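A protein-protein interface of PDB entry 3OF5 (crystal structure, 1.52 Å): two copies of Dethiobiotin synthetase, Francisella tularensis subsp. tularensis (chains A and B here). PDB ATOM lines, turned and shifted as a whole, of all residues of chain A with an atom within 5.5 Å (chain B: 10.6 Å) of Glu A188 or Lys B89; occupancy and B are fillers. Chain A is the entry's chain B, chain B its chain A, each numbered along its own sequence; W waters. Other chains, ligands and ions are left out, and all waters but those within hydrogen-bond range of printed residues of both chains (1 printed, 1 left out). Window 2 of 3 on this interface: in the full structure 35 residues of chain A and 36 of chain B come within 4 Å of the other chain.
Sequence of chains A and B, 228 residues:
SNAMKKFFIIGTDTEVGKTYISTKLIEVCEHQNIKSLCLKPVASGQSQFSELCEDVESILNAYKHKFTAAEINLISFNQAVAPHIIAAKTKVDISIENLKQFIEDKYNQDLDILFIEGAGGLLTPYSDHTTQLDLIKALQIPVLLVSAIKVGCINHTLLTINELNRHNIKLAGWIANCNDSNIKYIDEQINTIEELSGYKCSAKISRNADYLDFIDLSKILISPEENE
Hydrophobic or aromatic side chains of chain B that line the printed part of chain A: His B84, Ile B85, Ile B86 and Pro B125. Along chain B the printed residues that touch a printed residue of chain A span positions 79 to 125. Of the 10 printed residues of chain A, 5 touch a printed residue of chain B. Along chain A the printed residues that touch a printed residue of chain B span positions 154 to 192. Among the printed residues, 11 pairs touch across the chains. Among the printed residues, Asp or Glu carboxylates within 4 Å of a Lys or Arg side-chain nitrogen of the other chain: Glu A188 with Lys B89 (2.8 Å).
Of the printed residues of chain B, Tyr A185 touches Gln B79 (2.8 Å), Ile B85 (3.6 Å), Ile B86 (3.5 Å) and Lys B89 (3.9 Å). Gln A189 touches one residue of chain B. No residue of chain B comes within 4 Å of Asn A191. Of the printed residues of chain A, Ile B85 touches Tyr A185 (3.6 Å), Glu A188 (3.9 Å) and Gln A189 (3.5 Å). Of the printed residues of chain A, Ile B86 touches Tyr A185. Ala B87 touches none of the printed residues of chain A. Of the printed residues of chain A, Lys B89 touches Tyr A185 (3.9 Å) and Glu A188 (2.8 Å). Tyr B126 touches none of the printed residues of chain A. The nearest residue of chain B that does not touch Glu A188 is His B84 (5.0 Å).
Among the printed residues, pairs that only touch across the chains: Gln A189 with Ile B85 (3.5 Å), Ile A154 with Pro B125 (3.5 Å), Tyr A185 with Ile B86 (3.5 Å), Tyr A185 with Ile B85 (3.6 Å), Thr A192 with Pro B125 (3.7 Å), Ile A154 with His B84 (3.8 Å), Tyr A185 with Lys B89 (3.9 Å) and Glu A188 with Ile B85 (3.9 Å).
No position is printed for both chains. Of the 11 pairs that touch across the chains among the printed residues, none has its exchanged pair printed and touching as well.
The side-chain hydroxyl (OG1) of Thr A192 is in hydrogen-bond range of a ring nitrogen (NE2) of His B84, 2.8 Å away. NZ of Lys B89 lies within salt-bridge range of OE2 of Glu A188. The side-chain amide nitrogen (NE2) of Gln B79 is in hydrogen-bond range of the side-chain hydroxyl (OH) of Tyr A185 (2.8 Å).
Water W1 bridges OG1 of Thr A192 and NE2 of His B84.
The side-chain hydroxyl (OG1) of Thr A192 is in hydrogen-bond range of the backbone carbonyl oxygen (O) of Glu A188, at 2.8 Å. The backbone carbonyl oxygen of Ile B86 lies within hydrogen-bond range of the side-chain hydroxyl of Thr B90 (2.8 Å). The backbone carbonyl oxygen (O) of Tyr A185 is in hydrogen-bond range of the side-chain amide nitrogen (NE2) of Gln A189 (3.2 Å).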
ATOM      1  N   ILE A 154     -29.445  15.342  22.221  1.00  0.00           N
ATOM      2  CA  ILE A 154     -28.347  16.043  22.859  1.00  0.00           C
ATOM      3  C   ILE A 154     -28.911  16.992  23.899  1.00  0.00           C
ATOM      4  O   ILE A 154     -28.486  16.952  25.063  1.00  0.00           O
ATOM      5  CB  ILE A 154     -27.455  16.754  21.834  1.00  0.00           C
ATOM      6  CG1 ILE A 154     -26.923  15.753  20.793  1.00  0.00           C
ATOM      7  CG2 ILE A 154     -26.305  17.466  22.580  1.00  0.00           C
ATOM      8  CD1 ILE A 154     -26.297  16.462  19.526  1.00  0.00           C
ATOM      9  N   TYR A 185     -25.888  10.248  11.590  1.00  0.00           N
ATOM     10  CA  TYR A 185     -24.847  10.870  12.410  1.00  0.00           C
ATOM     11  C   TYR A 185     -24.866  10.465  13.865  1.00  0.00           C
ATOM     12  O   TYR A 185     -24.767  11.301  14.770  1.00  0.00           O
ATOM     13  CB  TYR A 185     -24.905  12.418  12.253  1.00  0.00           C
ATOM     14  CG  TYR A 185     -25.082  12.857  10.822  1.00  0.00           C
ATOM     15  CD1 TYR A 185     -24.068  12.678   9.889  1.00  0.00           C
ATOM     16  CD2 TYR A 185     -26.251  13.490  10.406  1.00  0.00           C
ATOM     17  CE1 TYR A 185     -24.205  13.136   8.577  1.00  0.00           C
ATOM     18  CE2 TYR A 185     -26.419  13.904   9.089  1.00  0.00           C
ATOM     19  CZ  TYR A 185     -25.388  13.740   8.183  1.00  0.00           C
ATOM     20  OH  TYR A 185     -25.542  14.193   6.898  1.00  0.00           O
ATOM     21  N   ILE A 186     -24.990   9.145  14.106  1.00  0.00           N
ATOM     22  CA  ILE A 186     -25.030   8.611  15.462  1.00  0.00           C
ATOM     23  C   ILE A 186     -23.746   8.889  16.212  1.00  0.00           C
ATOM     24  O   ILE A 186     -23.796   9.402  17.334  1.00  0.00           O
ATOM     25  CB  ILE A 186     -25.379   7.106  15.430  1.00  0.00           C
ATOM     26  CG1 ILE A 186     -26.851   6.904  15.011  1.00  0.00           C
ATOM     27  CG2 ILE A 186     -25.058   6.431  16.772  1.00  0.00           C
ATOM     28  CD1 ILE A 186     -27.230   5.407  14.682  1.00  0.00           C
ATOM     29  N   ASP A 187     -22.604   8.602  15.576  1.00  0.00           N
ATOM     30  CA  ASP A 187     -21.290   8.827  16.165  1.00  0.00           C
ATOM     31  C   ASP A 187     -21.059  10.309  16.493  1.00  0.00           C
ATOM     32  O   ASP A 187     -20.513  10.603  17.549  1.00  0.00           O
ATOM     33  CB  ASP A 187     -20.185   8.268  15.249  1.00  0.00           C
ATOM     34  CG  ASP A 187     -20.288   8.647  13.783  1.00  0.00           C
ATOM     35  OD1 ASP A 187     -21.291   8.241  13.121  1.00  0.00           O
ATOM     36  OD2 ASP A 187     -19.347   9.298  13.271  1.00  0.00           O
ATOM     37  N   GLU A 188     -21.525  11.226  15.621  1.00  0.00           N
ATOM     38  CA  GLU A 188     -21.383  12.677  15.813  1.00  0.00           C
ATOM     39  C   GLU A 188     -22.230  13.138  16.990  1.00  0.00           C
ATOM     40  O   GLU A 188     -21.775  13.973  17.771  1.00  0.00           O
ATOM     41  CB  GLU A 188     -21.819  13.419  14.555  1.00  0.00           C
ATOM     42  CG  GLU A 188     -20.832  13.291  13.408  1.00  0.00           C
ATOM     43  CD  GLU A 188     -20.935  12.061  12.531  1.00  0.00           C
ATOM     44  OE1 GLU A 188     -21.763  11.160  12.805  1.00  0.00           O
ATOM     45  OE2 GLU A 188     -20.132  11.975  11.574  1.00  0.00           O
ATOM     46  N   GLN A 189     -23.441  12.574  17.154  1.00  0.00           N
ATOM     47  CA  GLN A 189     -24.289  12.959  18.288  1.00  0.00           C
ATOM     48  C   GLN A 189     -23.651  12.501  19.599  1.00  0.00           C
ATOM     49  O   GLN A 189     -23.595  13.275  20.569  1.00  0.00           O
ATOM     50  CB  GLN A 189     -25.680  12.356  18.137  1.00  0.00           C
ATOM     51  CG  GLN A 189     -26.442  13.004  16.991  1.00  0.00           C
ATOM     52  CD  GLN A 189     -27.762  12.335  16.786  1.00  0.00           C
ATOM     53  OE1 GLN A 189     -28.707  12.522  17.568  1.00  0.00           O
ATOM     54  NE2 GLN A 189     -27.841  11.483  15.762  1.00  0.00           N
ATOM     55  N   ILE A 190     -23.133  11.252  19.630  1.00  0.00           N
ATOM     56  CA  ILE A 190     -22.451  10.745  20.822  1.00  0.00           C
ATOM     57  C   ILE A 190     -21.225  11.606  21.155  1.00  0.00           C
ATOM     58  O   ILE A 190     -21.057  12.015  22.310  1.00  0.00           O
ATOM     59  CB  ILE A 190     -22.063   9.268  20.610  1.00  0.00           C
ATOM     60  CG1 ILE A 190     -23.326   8.399  20.528  1.00  0.00           C
ATOM     61  CG2 ILE A 190     -21.155   8.758  21.751  1.00  0.00           C
ATOM     62  CD1 ILE A 190     -23.083   6.977  20.020  1.00  0.00           C
ATOM     63  N   ASN A 191     -20.414  11.933  20.140  1.00  0.00           N
ATOM     64  CA  ASN A 191     -19.212  12.732  20.367  1.00  0.00           C
ATOM     65  C   ASN A 191     -19.601  14.107  20.920  1.00  0.00           C
ATOM     66  O   ASN A 191     -18.922  14.614  21.802  1.00  0.00           O
ATOM     67  CB  ASN A 191     -18.439  12.893  19.065  1.00  0.00           C
ATOM     68  CG  ASN A 191     -17.154  13.662  19.214  1.00  0.00           C
ATOM     69  OD1 ASN A 191     -17.062  14.828  18.835  1.00  0.00           O
ATOM     70  ND2 ASN A 191     -16.147  13.030  19.782  1.00  0.00           N
ATOM     71  N   THR A 192     -20.701  14.703  20.413  1.00  0.00           N
ATOM     72  CA  THR A 192     -21.127  16.015  20.912  1.00  0.00           C
ATOM     73  C   THR A 192     -21.544  15.940  22.383  1.00  0.00           C
ATOM     74  O   THR A 192     -21.152  16.803  23.182  1.00  0.00           O
ATOM     75  CB  THR A 192     -22.242  16.565  20.040  1.00  0.00           C
ATOM     76  OG1 THR A 192     -21.756  16.647  18.699  1.00  0.00           O
ATOM     77  CG2 THR A 192     -22.664  17.961  20.484  1.00  0.00           C
ATOM     78  N   ILE A 193     -22.320  14.917  22.748  1.00  0.00           N
ATOM     79  CA  ILE A 193     -22.716  14.792  24.142  1.00  0.00           C
ATOM     80  C   ILE A 193     -21.459  14.653  25.016  1.00  0.00           C
ATOM     81  O   ILE A 193     -21.396  15.259  26.092  1.00  0.00           O
ATOM     82  CB  ILE A 193     -23.645  13.584  24.328  1.00  0.00           C
ATOM     83  CG1 ILE A 193     -24.998  13.840  23.638  1.00  0.00           C
ATOM     84  CG2 ILE A 193     -23.849  13.293  25.834  1.00  0.00           C
ATOM     85  CD1 ILE A 193     -25.903  12.583  23.528  1.00  0.00           C
ATOM     86  N   PHE B  77     -30.144  24.943   6.689  1.00  0.00           N
ATOM     87  CA  PHE B  77     -29.675  23.594   6.331  1.00  0.00           C
ATOM     88  C   PHE B  77     -30.837  22.801   5.775  1.00  0.00           C
ATOM     89  O   PHE B  77     -31.951  22.898   6.293  1.00  0.00           O
ATOM     90  CB  PHE B  77     -29.068  22.869   7.551  1.00  0.00           C
ATOM     91  CG  PHE B  77     -27.921  23.614   8.189  1.00  0.00           C
ATOM     92  CD1 PHE B  77     -26.701  23.749   7.527  1.00  0.00           C
ATOM     93  CD2 PHE B  77     -28.061  24.192   9.437  1.00  0.00           C
ATOM     94  CE1 PHE B  77     -25.633  24.423   8.121  1.00  0.00           C
ATOM     95  CE2 PHE B  77     -26.994  24.880  10.029  1.00  0.00           C
ATOM     96  CZ  PHE B  77     -25.784  24.975   9.368  1.00  0.00           C
ATOM     97  N   GLN B  79     -31.159  19.336   5.697  1.00  0.00           N
ATOM     98  CA  GLN B  79     -31.451  18.160   6.510  1.00  0.00           C
ATOM     99  C   GLN B  79     -32.037  18.497   7.863  1.00  0.00           C
ATOM    100  O   GLN B  79     -31.532  19.379   8.549  1.00  0.00           O
ATOM    101  CB  GLN B  79     -30.189  17.313   6.712  1.00  0.00           C
ATOM    102  CG  GLN B  79     -29.761  16.528   5.492  1.00  0.00           C
ATOM    103  CD  GLN B  79     -28.721  15.520   5.905  1.00  0.00           C
ATOM    104  OE1 GLN B  79     -29.021  14.518   6.550  1.00  0.00           O
ATOM    105  NE2 GLN B  79     -27.476  15.779   5.560  1.00  0.00           N
ATOM    106  N   VAL B  81     -31.749  17.498  10.914  1.00  0.00           N
ATOM    107  CA  VAL B  81     -30.912  16.868  11.942  1.00  0.00           C
ATOM    108  C   VAL B  81     -30.309  17.991  12.788  1.00  0.00           C
ATOM    109  O   VAL B  81     -30.545  19.163  12.487  1.00  0.00           O
ATOM    110  CB  VAL B  81     -29.805  15.968  11.337  1.00  0.00           C
ATOM    111  CG1 VAL B  81     -30.387  14.794  10.536  1.00  0.00           C
ATOM    112  CG2 VAL B  81     -28.850  16.783  10.483  1.00  0.00           C
ATOM    113  N   ALA B  82     -29.526  17.651  13.841  1.00  0.00           N
ATOM    114  CA  ALA B  82     -28.900  18.654  14.709  1.00  0.00           C
ATOM    115  C   ALA B  82     -28.151  19.657  13.820  1.00  0.00           C
ATOM    116  O   ALA B  82     -27.305  19.230  13.019  1.00  0.00           O
ATOM    117  CB  ALA B  82     -27.937  17.969  15.659  1.00  0.00           C
ATOM    118  N   PRO B  83     -28.483  20.968  13.862  1.00  0.00           N
ATOM    119  CA  PRO B  83     -27.836  21.902  12.915  1.00  0.00           C
ATOM    120  C   PRO B  83     -26.320  21.973  13.026  1.00  0.00           C
ATOM    121  O   PRO B  83     -25.659  22.144  12.010  1.00  0.00           O
ATOM    122  CB  PRO B  83     -28.495  23.254  13.214  1.00  0.00           C
ATOM    123  CG  PRO B  83     -29.044  23.108  14.608  1.00  0.00           C
ATOM    124  CD  PRO B  83     -29.490  21.662  14.694  1.00  0.00           C
ATOM    125  N   HIS B  84     -25.762  21.781  14.217  1.00  0.00           N
ATOM    126  CA  HIS B  84     -24.313  21.848  14.326  1.00  0.00           C
ATOM    127  C   HIS B  84     -23.629  20.722  13.591  1.00  0.00           C
ATOM    128  O   HIS B  84     -22.478  20.883  13.201  1.00  0.00           O
ATOM    129  CB  HIS B  84     -23.825  21.951  15.786  1.00  0.00           C
ATOM    130  CG  HIS B  84     -23.593  20.640  16.458  1.00  0.00           C
ATOM    131  ND1 HIS B  84     -24.648  19.839  16.840  1.00  0.00           N
ATOM    132  CD2 HIS B  84     -22.436  20.002  16.728  1.00  0.00           C
ATOM    133  CE1 HIS B  84     -24.101  18.749  17.346  1.00  0.00           C
ATOM    134  NE2 HIS B  84     -22.776  18.797  17.288  1.00  0.00           N
ATOM    135  N   ILE B  85     -24.310  19.564  13.455  1.00  0.00           N
ATOM    136  CA  ILE B  85     -23.705  18.422  12.768  1.00  0.00           C
ATOM    137  C   ILE B  85     -23.568  18.746  11.284  1.00  0.00           C
ATOM    138  O   ILE B  85     -22.486  18.569  10.726  1.00  0.00           O
ATOM    139  CB  ILE B  85     -24.491  17.131  13.030  1.00  0.00           C
ATOM    140  CG1 ILE B  85     -24.251  16.711  14.487  1.00  0.00           C
ATOM    141  CG2 ILE B  85     -24.010  16.013  12.074  1.00  0.00           C
ATOM    142  CD1 ILE B  85     -25.061  15.557  15.020  1.00  0.00           C
ATOM    143  N   ILE B  86     -24.646  19.277  10.649  1.00  0.00           N
ATOM    144  CA  ILE B  86     -24.573  19.656   9.227  1.00  0.00           C
ATOM    145  C   ILE B  86     -23.588  20.772   9.036  1.00  0.00           C
ATOM    146  O   ILE B  86     -22.811  20.744   8.075  1.00  0.00           O
ATOM    147  CB  ILE B  86     -25.956  20.001   8.611  1.00  0.00           C
ATOM    148  CG1 ILE B  86     -26.887  18.796   8.685  1.00  0.00           C
ATOM    149  CG2 ILE B  86     -25.826  20.474   7.146  1.00  0.00           C
ATOM    150  CD1 ILE B  86     -26.256  17.409   8.188  1.00  0.00           C
ATOM    151  N   ALA B  87     -23.580  21.728   9.975  1.00  0.00           N
ATOM    152  CA  ALA B  87     -22.674  22.878   9.914  1.00  0.00           C
ATOM    153  C   ALA B  87     -21.226  22.356   9.825  1.00  0.00           C
ATOM    154  O   ALA B  87     -20.492  22.736   8.906  1.00  0.00           O
ATOM    155  CB  ALA B  87     -22.842  23.754  11.144  1.00  0.00           C
ATOM    156  N   ALA B  88     -20.858  21.407  10.713  1.00  0.00           N
ATOM    157  CA  ALA B  88     -19.511  20.816  10.696  1.00  0.00           C
ATOM    158  C   ALA B  88     -19.210  20.053   9.403  1.00  0.00           C
ATOM    159  O   ALA B  88     -18.083  20.145   8.906  1.00  0.00           O
ATOM    160  CB  ALA B  88     -19.302  19.927  11.912  1.00  0.00           C
ATOM    161  N   LYS B  89     -20.216  19.372   8.813  1.00  0.00           N
ATOM    162  CA  LYS B  89     -20.035  18.621   7.557  1.00  0.00           C
ATOM    163  C   LYS B  89     -19.945  19.539   6.341  1.00  0.00           C
ATOM    164  O   LYS B  89     -19.310  19.169   5.350  1.00  0.00           O
ATOM    165  CB  LYS B  89     -21.198  17.635   7.322  1.00  0.00           C
ATOM    166  CG  LYS B  89     -21.375  16.553   8.382  1.00  0.00           C
ATOM    167  CD  LYS B  89     -20.462  15.387   8.181  1.00  0.00           C
ATOM    168  CE  LYS B  89     -20.621  14.396   9.314  1.00  0.00           C
ATOM    169  NZ  LYS B  89     -19.569  13.367   9.222  1.00  0.00           N
ATOM    170  N   THR B  90     -20.574  20.726   6.405  1.00  0.00           N
ATOM    171  CA  THR B  90     -20.620  21.658   5.276  1.00  0.00           C
ATOM    172  C   THR B  90     -19.742  22.890   5.425  1.00  0.00           C
ATOM    173  O   THR B  90     -19.890  23.840   4.643  1.00  0.00           O
ATOM    174  CB  THR B  90     -22.066  22.004   4.912  1.00  0.00           C
ATOM    175  OG1 THR B  90     -22.678  22.676   6.018  1.00  0.00           O
ATOM    176  CG2 THR B  90     -22.886  20.777   4.494  1.00  0.00           C
ATOM    177  N   LYS B  91     -18.828  22.887   6.424  1.00  0.00           N
ATOM    178  CA  LYS B  91     -17.888  23.985   6.701  1.00  0.00           C
ATOM    179  C   LYS B  91     -18.564  25.331   6.974  1.00  0.00           C
ATOM    180  O   LYS B  91     -18.106  26.383   6.514  1.00  0.00           O
ATOM    181  CB  LYS B  91     -16.791  24.082   5.631  1.00  0.00           C
ATOM    182  CG  LYS B  91     -15.765  22.958   5.716  1.00  0.00           C
ATOM    183  CD  LYS B  91     -14.725  23.082   4.617  1.00  0.00           C
ATOM    184  CE  LYS B  91     -13.451  22.362   4.976  1.00  0.00           C
ATOM    185  NZ  LYS B  91     -12.460  22.405   3.869  1.00  0.00           N
ATOM    186  N   VAL B  92     -19.678  25.271   7.704  1.00  0.00           N
ATOM    187  CA  VAL B  92     -20.449  26.435   8.141  1.00  0.00           C
ATOM    188  C   VAL B  92     -20.226  26.555   9.656  1.00  0.00           C
ATOM    189  O   VAL B  92     -20.358  25.566  10.377  1.00  0.00           O
ATOM    190  CB  VAL B  92     -21.964  26.281   7.790  1.00  0.00           C
ATOM    191  CG1 VAL B  92     -22.826  27.362   8.455  1.00  0.00           C
ATOM    192  CG2 VAL B  92     -22.183  26.278   6.277  1.00  0.00           C
ATOM    193  N   ASP B  93     -19.850  27.747  10.103  1.00  0.00           N
ATOM    194  CA  ASP B  93     -19.668  28.061  11.510  1.00  0.00           C
ATOM    195  C   ASP B  93     -20.976  28.676  11.985  1.00  0.00           C
ATOM    196  O   ASP B  93     -21.439  29.659  11.393  1.00  0.00           O
ATOM    197  CB  ASP B  93     -18.521  29.084  11.674  1.00  0.00           C
ATOM    198  CG  ASP B  93     -17.981  29.302  13.083  1.00  0.00           C
ATOM    199  OD1 ASP B  93     -18.706  29.008  14.056  1.00  0.00           O
ATOM    200  OD2 ASP B  93     -16.847  29.819  13.209  1.00  0.00           O
ATOM    201  N   ILE B  94     -21.602  28.092  13.015  1.00  0.00           N
ATOM    202  CA  ILE B  94     -22.789  28.710  13.615  1.00  0.00           C
ATOM    203  C   ILE B  94     -22.195  29.466  14.801  1.00  0.00           C
ATOM    204  O   ILE B  94     -21.896  28.849  15.816  1.00  0.00           O
ATOM    205  CB  ILE B  94     -23.894  27.738  14.069  1.00  0.00           C
ATOM    206  CG1 ILE B  94     -24.353  26.796  12.935  1.00  0.00           C
ATOM    207  CG2 ILE B  94     -25.084  28.532  14.649  1.00  0.00           C
ATOM    208  CD1 ILE B  94     -25.255  25.683  13.448  1.00  0.00           C
ATOM    209  N   PRO B 125     -27.117  22.040  20.499  1.00  0.00           N
ATOM    210  CA  PRO B 125     -25.827  22.673  20.205  1.00  0.00           C
ATOM    211  C   PRO B 125     -25.822  23.577  18.988  1.00  0.00           C
ATOM    212  O   PRO B 125     -26.534  23.337  18.017  1.00  0.00           O
ATOM    213  CB  PRO B 125     -24.897  21.479  19.958  1.00  0.00           C
ATOM    214  CG  PRO B 125     -25.567  20.315  20.629  1.00  0.00           C
ATOM    215  CD  PRO B 125     -27.037  20.572  20.343  1.00  0.00           C
ATOM    216  N   TYR B 126     -24.981  24.620  19.041  1.00  0.00           N
ATOM    217  CA  TYR B 126     -24.698  25.394  17.844  1.00  0.00           C
ATOM    218  C   TYR B 126     -23.291  24.993  17.349  1.00  0.00           C
ATOM    219  O   TYR B 126     -22.909  25.320  16.225  1.00  0.00           O
ATOM    220  CB  TYR B 126     -24.722  26.887  18.130  1.00  0.00           C
ATOM    221  CG  TYR B 126     -26.095  27.519  18.226  1.00  0.00           C
ATOM    222  CD1 TYR B 126     -27.225  26.869  17.743  1.00  0.00           C
ATOM    223  CD2 TYR B 126     -26.253  28.796  18.742  1.00  0.00           C
ATOM    224  CE1 TYR B 126     -28.483  27.486  17.768  1.00  0.00           C
ATOM    225  CE2 TYR B 126     -27.502  29.399  18.815  1.00  0.00           C
ATOM    226  CZ  TYR B 126     -28.606  28.763  18.288  1.00  0.00           C
ATOM    227  OH  TYR B 126     -29.837  29.372  18.370  1.00  0.00           O
ATOM    228  N   SER B 127     -22.516  24.281  18.194  1.00  0.00           N
ATOM    229  CA  SER B 127     -21.170  23.801  17.876  1.00  0.00           C
ATOM    230  C   SER B 127     -20.793  22.743  18.914  1.00  0.00           C
ATOM    231  O   SER B 127     -21.576  22.456  19.838  1.00  0.00           O
ATOM    232  CB  SER B 127     -20.160  24.953  17.909  1.00  0.00           C
ATOM    233  OG  SER B 127     -19.930  25.358  19.249  1.00  0.00           O
ATOM    234  N   ASP B 128     -19.548  22.271  18.854  1.00  0.00           N
ATOM    235  CA  ASP B 128     -19.055  21.322  19.842  1.00  0.00           C
ATOM    236  C   ASP B 128     -18.789  21.985  21.201  1.00  0.00           C
ATOM    237  O   ASP B 128     -18.422  21.275  22.144  1.00  0.00           O
ATOM    238  CB  ASP B 128     -17.759  20.666  19.321  1.00  0.00           C
ATOM    239  CG  ASP B 128     -16.558  21.576  19.084  1.00  0.00           C
ATOM    240  OD1 ASP B 128     -16.734  22.820  19.023  1.00  0.00           O
ATOM    241  OD2 ASP B 128     -15.469  21.050  18.844  1.00  0.00           O
ATOM    242  N   HIS B 129     -18.980  23.327  21.322  1.00  0.00           N
ATOM    243  CA  HIS B 129     -18.718  24.014  22.592  1.00  0.00           C
ATOM    244  C   HIS B 129     -19.776  25.026  22.995  1.00  0.00           C
ATOM    245  O   HIS B 129     -19.617  25.696  24.013  1.00  0.00           O
ATOM    246  CB  HIS B 129     -17.336  24.676  22.569  1.00  0.00           C
ATOM    247  CG  HIS B 129     -17.234  25.794  21.589  1.00  0.00           C
ATOM    248  ND1 HIS B 129     -17.021  25.559  20.233  1.00  0.00           N
ATOM    249  CD2 HIS B 129     -17.284  27.131  21.796  1.00  0.00           C
ATOM    250  CE1 HIS B 129     -17.015  26.752  19.661  1.00  0.00           C
ATOM    251  NE2 HIS B 129     -17.177  27.728  20.559  1.00  0.00           N
HETATM  252  O   HOH W   1     -19.681  18.267  17.992  1.00  0.00           O
